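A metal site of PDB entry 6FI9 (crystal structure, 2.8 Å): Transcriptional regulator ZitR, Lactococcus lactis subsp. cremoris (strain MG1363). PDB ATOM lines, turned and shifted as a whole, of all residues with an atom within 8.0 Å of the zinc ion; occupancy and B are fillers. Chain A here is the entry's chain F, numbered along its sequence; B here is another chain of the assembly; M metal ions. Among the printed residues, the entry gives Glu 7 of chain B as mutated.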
ATOM      1  N   HIS A  21      30.834 -17.047  11.500  1.00  0.00           N
ATOM      2  CA  HIS A  21      31.036 -15.602  11.383  1.00  0.00           C
ATOM      3  C   HIS A  21      31.518 -15.010  12.709  1.00  0.00           C
ATOM      4  O   HIS A  21      32.321 -14.074  12.722  1.00  0.00           O
ATOM      5  CB  HIS A  21      29.750 -14.895  10.920  1.00  0.00           C
ATOM      6  CG  HIS A  21      29.473 -15.034   9.456  1.00  0.00           C
ATOM      7  ND1 HIS A  21      28.706 -16.074   8.952  1.00  0.00           N
ATOM      8  CD2 HIS A  21      29.880 -14.255   8.423  1.00  0.00           C
ATOM      9  CE1 HIS A  21      28.664 -15.888   7.656  1.00  0.00           C
ATOM     10  NE2 HIS A  21      29.355 -14.809   7.280  1.00  0.00           N
ATOM     11  N   GLU A  22      31.013 -15.568  13.829  1.00  0.00           N
ATOM     12  CA  GLU A  22      31.335 -15.171  15.208  1.00  0.00           C
ATOM     13  C   GLU A  22      31.776 -16.364  16.061  1.00  0.00           C
ATOM     14  O   GLU A  22      31.398 -17.502  15.776  1.00  0.00           O
ATOM     15  CB  GLU A  22      30.147 -14.441  15.860  1.00  0.00           C
ATOM     16  CG  GLU A  22      28.862 -15.260  15.931  1.00  0.00           C
ATOM     17  CD  GLU A  22      27.648 -14.529  16.477  1.00  0.00           C
ATOM     18  OE1 GLU A  22      27.741 -14.008  17.611  1.00  0.00           O
ATOM     19  OE2 GLU A  22      26.612 -14.493  15.776  1.00  0.00           O
ATOM     20  N   ILE A  23      32.569 -16.106  17.128  1.00  0.00           N
ATOM     21  CA  ILE A  23      33.054 -17.126  18.047  1.00  0.00           C
ATOM     22  C   ILE A  23      32.175 -17.181  19.300  1.00  0.00           C
ATOM     23  O   ILE A  23      32.006 -16.167  20.000  1.00  0.00           O
ATOM     24  CB  ILE A  23      34.585 -16.984  18.354  1.00  0.00           C
ATOM     25  CG1 ILE A  23      35.416 -17.419  17.125  1.00  0.00           C
ATOM     26  CG2 ILE A  23      34.997 -17.784  19.603  1.00  0.00           C
ATOM     27  CD1 ILE A  23      36.830 -16.841  17.059  1.00  0.00           C
ATOM     28  N   LEU A  24      31.594 -18.360  19.557  1.00  0.00           N
ATOM     29  CA  LEU A  24      30.733 -18.636  20.705  1.00  0.00           C
ATOM     30  C   LEU A  24      31.046 -20.050  21.229  1.00  0.00           C
ATOM     31  O   LEU A  24      30.779 -21.038  20.533  1.00  0.00           O
ATOM     32  CB  LEU A  24      29.242 -18.523  20.321  1.00  0.00           C
ATOM     33  CG  LEU A  24      28.681 -17.124  20.115  1.00  0.00           C
ATOM     34  CD1 LEU A  24      27.673 -17.125  18.993  1.00  0.00           C
ATOM     35  CD2 LEU A  24      28.034 -16.600  21.368  1.00  0.00           C
ATOM     36  N   SER A  36      24.405 -18.805  13.020  1.00  0.00           N
ATOM     37  CA  SER A  36      25.059 -17.891  13.964  1.00  0.00           C
ATOM     38  C   SER A  36      24.496 -16.468  13.832  1.00  0.00           C
ATOM     39  O   SER A  36      24.019 -15.904  14.814  1.00  0.00           O
ATOM     40  CB  SER A  36      26.575 -17.893  13.767  1.00  0.00           C
ATOM     41  OG  SER A  36      27.125 -19.188  13.914  1.00  0.00           O
ATOM     42  N   THR A  37      24.533 -15.921  12.598  1.00  0.00           N
ATOM     43  CA  THR A  37      24.057 -14.580  12.260  1.00  0.00           C
ATOM     44  C   THR A  37      22.547 -14.435  12.461  1.00  0.00           C
ATOM     45  O   THR A  37      22.120 -13.446  13.070  1.00  0.00           O
ATOM     46  CB  THR A  37      24.501 -14.174  10.840  1.00  0.00           C
ATOM     47  OG1 THR A  37      24.020 -15.141   9.902  1.00  0.00           O
ATOM     48  CG2 THR A  37      26.016 -14.006  10.709  1.00  0.00           C
ATOM     49  N   GLU A  39      20.421 -16.003  14.468  1.00  0.00           N
ATOM     50  CA  GLU A  39      20.103 -15.939  15.886  1.00  0.00           C
ATOM     51  C   GLU A  39      20.566 -14.617  16.515  1.00  0.00           C
ATOM     52  O   GLU A  39      19.933 -14.138  17.464  1.00  0.00           O
ATOM     53  CB  GLU A  39      20.698 -17.140  16.631  1.00  0.00           C
ATOM     54  CG  GLU A  39      19.856 -18.407  16.526  1.00  0.00           C
ATOM     55  CD  GLU A  39      20.401 -19.593  17.284  1.00  0.00           C
ATOM     56  OE1 GLU A  39      20.341 -19.569  18.536  1.00  0.00           O
ATOM     57  OE2 GLU A  39      20.871 -20.549  16.636  1.00  0.00           O
ATOM     58  N   HIS A  40      21.662 -14.035  15.988  1.00  0.00           N
ATOM     59  CA  HIS A  40      22.214 -12.753  16.456  1.00  0.00           C
ATOM     60  C   HIS A  40      21.336 -11.575  16.010  1.00  0.00           C
ATOM     61  O   HIS A  40      21.288 -10.565  16.713  1.00  0.00           O
ATOM     62  CB  HIS A  40      23.671 -12.565  15.990  1.00  0.00           C
ATOM     63  CG  HIS A  40      24.368 -11.410  16.649  1.00  0.00           C
ATOM     64  ND1 HIS A  40      24.921 -11.528  17.912  1.00  0.00           N
ATOM     65  CD2 HIS A  40      24.561 -10.157  16.191  1.00  0.00           C
ATOM     66  CE1 HIS A  40      25.435 -10.336  18.176  1.00  0.00           C
ATOM     67  NE2 HIS A  40      25.250  -9.475  17.174  1.00  0.00           N
ATOM     68  N   ILE A  41      20.648 -11.714  14.855  1.00  0.00           N
ATOM     69  CA  ILE A  41      19.739 -10.692  14.319  1.00  0.00           C
ATOM     70  C   ILE A  41      18.538 -10.554  15.273  1.00  0.00           C
ATOM     71  O   ILE A  41      18.133  -9.435  15.581  1.00  0.00           O
ATOM     72  CB  ILE A  41      19.341 -10.987  12.834  1.00  0.00           C
ATOM     73  CG1 ILE A  41      20.561 -10.820  11.898  1.00  0.00           C
ATOM     74  CG2 ILE A  41      18.196 -10.074  12.358  1.00  0.00           C
ATOM     75  CD1 ILE A  41      20.537 -11.662  10.614  1.00  0.00           C
ATOM     76  N   MET A  43      18.528 -11.267  18.491  1.00  0.00           N
ATOM     77  CA  MET A  43      19.081 -10.734  19.735  1.00  0.00           C
ATOM     78  C   MET A  43      19.084  -9.190  19.760  1.00  0.00           C
ATOM     79  O   MET A  43      18.596  -8.602  20.720  1.00  0.00           O
ATOM     80  CB  MET A  43      20.486 -11.306  19.993  1.00  0.00           C
ATOM     81  CG  MET A  43      21.078 -10.929  21.344  1.00  0.00           C
ATOM     82  SD  MET A  43      22.843 -11.260  21.443  1.00  0.00           S
ATOM     83  CE  MET A  43      23.290 -10.214  22.798  1.00  0.00           C
ATOM     84  N   ILE A  44      19.624  -8.549  18.691  1.00  0.00           N
ATOM     85  CA  ILE A  44      19.709  -7.089  18.564  1.00  0.00           C
ATOM     86  C   ILE A  44      18.327  -6.450  18.335  1.00  0.00           C
ATOM     87  O   ILE A  44      18.121  -5.295  18.718  1.00  0.00           O
ATOM     88  CB  ILE A  44      20.760  -6.611  17.529  1.00  0.00           C
ATOM     89  CG1 ILE A  44      20.521  -7.201  16.119  1.00  0.00           C
ATOM     90  CG2 ILE A  44      22.192  -6.874  18.017  1.00  0.00           C
ATOM     91  CD1 ILE A  44      20.858  -6.268  14.974  1.00  0.00           C
ATOM     92  N   LEU A  59      25.929  -6.098  12.821  1.00  0.00           N
ATOM     93  CA  LEU A  59      26.520  -7.394  12.482  1.00  0.00           C
ATOM     94  C   LEU A  59      27.829  -7.317  11.695  1.00  0.00           C
ATOM     95  O   LEU A  59      28.557  -8.307  11.629  1.00  0.00           O
ATOM     96  CB  LEU A  59      25.498  -8.258  11.721  1.00  0.00           C
ATOM     97  CG  LEU A  59      24.616  -9.167  12.572  1.00  0.00           C
ATOM     98  CD1 LEU A  59      23.337  -8.454  13.000  1.00  0.00           C
ATOM     99  CD2 LEU A  59      24.271 -10.420  11.802  1.00  0.00           C
ATOM    100  N   HIS A 106      20.274 -16.521  22.955  1.00  0.00           N
ATOM    101  CA  HIS A 106      21.432 -15.923  22.281  1.00  0.00           C
ATOM    102  C   HIS A 106      22.109 -14.847  23.150  1.00  0.00           C
ATOM    103  O   HIS A 106      23.329 -14.698  23.072  1.00  0.00           O
ATOM    104  CB  HIS A 106      21.057 -15.369  20.908  1.00  0.00           C
ATOM    105  CG  HIS A 106      22.204 -15.344  19.945  1.00  0.00           C
ATOM    106  ND1 HIS A 106      22.600 -16.483  19.270  1.00  0.00           N
ATOM    107  CD2 HIS A 106      23.014 -14.325  19.591  1.00  0.00           C
ATOM    108  CE1 HIS A 106      23.624 -16.124  18.525  1.00  0.00           C
ATOM    109  NE2 HIS A 106      23.909 -14.827  18.676  1.00  0.00           N
ATOM    110  N   ALA A 107      21.319 -14.112  23.970  1.00  0.00           N
ATOM    111  CA  ALA A 107      21.827 -13.076  24.883  1.00  0.00           C
ATOM    112  C   ALA A 107      22.558 -13.711  26.070  1.00  0.00           C
ATOM    113  O   ALA A 107      23.455 -13.082  26.651  1.00  0.00           O
ATOM    114  CB  ALA A 107      20.691 -12.206  25.377  1.00  0.00           C
ATOM    115  N   HIS A 109      23.943 -17.051  25.754  1.00  0.00           N
ATOM    116  CA  HIS A 109      25.036 -17.853  25.174  1.00  0.00           C
ATOM    117  C   HIS A 109      26.265 -16.978  24.882  1.00  0.00           C
ATOM    118  O   HIS A 109      27.382 -17.481  24.896  1.00  0.00           O
ATOM    119  CB  HIS A 109      24.586 -18.615  23.924  1.00  0.00           C
ATOM    120  CG  HIS A 109      25.549 -19.683  23.487  1.00  0.00           C
ATOM    121  ND1 HIS A 109      26.311 -19.547  22.344  1.00  0.00           N
ATOM    122  CD2 HIS A 109      25.870 -20.856  24.088  1.00  0.00           C
ATOM    123  CE1 HIS A 109      27.049 -20.637  22.270  1.00  0.00           C
ATOM    124  NE2 HIS A 109      26.819 -21.457  23.302  1.00  0.00           N
ATOM    125  N   HIS A 110      26.037 -15.671  24.626  1.00  0.00           N
ATOM    126  CA  HIS A 110      27.099 -14.689  24.414  1.00  0.00           C
ATOM    127  C   HIS A 110      27.703 -14.366  25.780  1.00  0.00           C
ATOM    128  O   HIS A 110      28.910 -14.177  25.889  1.00  0.00           O
ATOM    129  CB  HIS A 110      26.557 -13.412  23.750  1.00  0.00           C
ATOM    130  CG  HIS A 110      27.097 -13.193  22.366  1.00  0.00           C
ATOM    131  ND1 HIS A 110      28.406 -12.784  22.158  1.00  0.00           N
ATOM    132  CD2 HIS A 110      26.476 -13.310  21.170  1.00  0.00           C
ATOM    133  CE1 HIS A 110      28.535 -12.687  20.845  1.00  0.00           C
ATOM    134  NE2 HIS A 110      27.405 -12.988  20.206  1.00  0.00           N
ATOM    135  N   GLU B   7      37.042 -11.152  23.141  1.00  0.00           N
ATOM    136  CA  GLU B   7      35.975 -11.247  22.149  1.00  0.00           C
ATOM    137  C   GLU B   7      36.249 -10.315  20.949  1.00  0.00           C
ATOM    138  O   GLU B   7      36.034 -10.718  19.806  1.00  0.00           O
ATOM    139  CB  GLU B   7      34.605 -10.935  22.785  1.00  0.00           C
ATOM    140  CG  GLU B   7      33.421 -11.365  21.926  1.00  0.00           C
ATOM    141  CD  GLU B   7      32.061 -11.078  22.538  1.00  0.00           C
ATOM    142  OE1 GLU B   7      31.747  -9.893  22.760  1.00  0.00           O
ATOM    143  OE2 GLU B   7      31.294 -12.045  22.766  1.00  0.00           O
HETATM  144 ZN    ZN M   1      26.489 -12.775  18.288  1.00  0.00          ZN
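A ring nitrogen (ND1) of His 110 is in hydrogen-bond range of the side-chain carboxylate of Glu 7 of chain B.
Merely in contact with the zinc ion: His 106 (3.3 Å).
The zinc ion is bound by the side-chain carboxylate (OE1) of Glu 22, a ring nitrogen (ND1) of His 40 and a ring nitrogen (NE2) of His 110.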
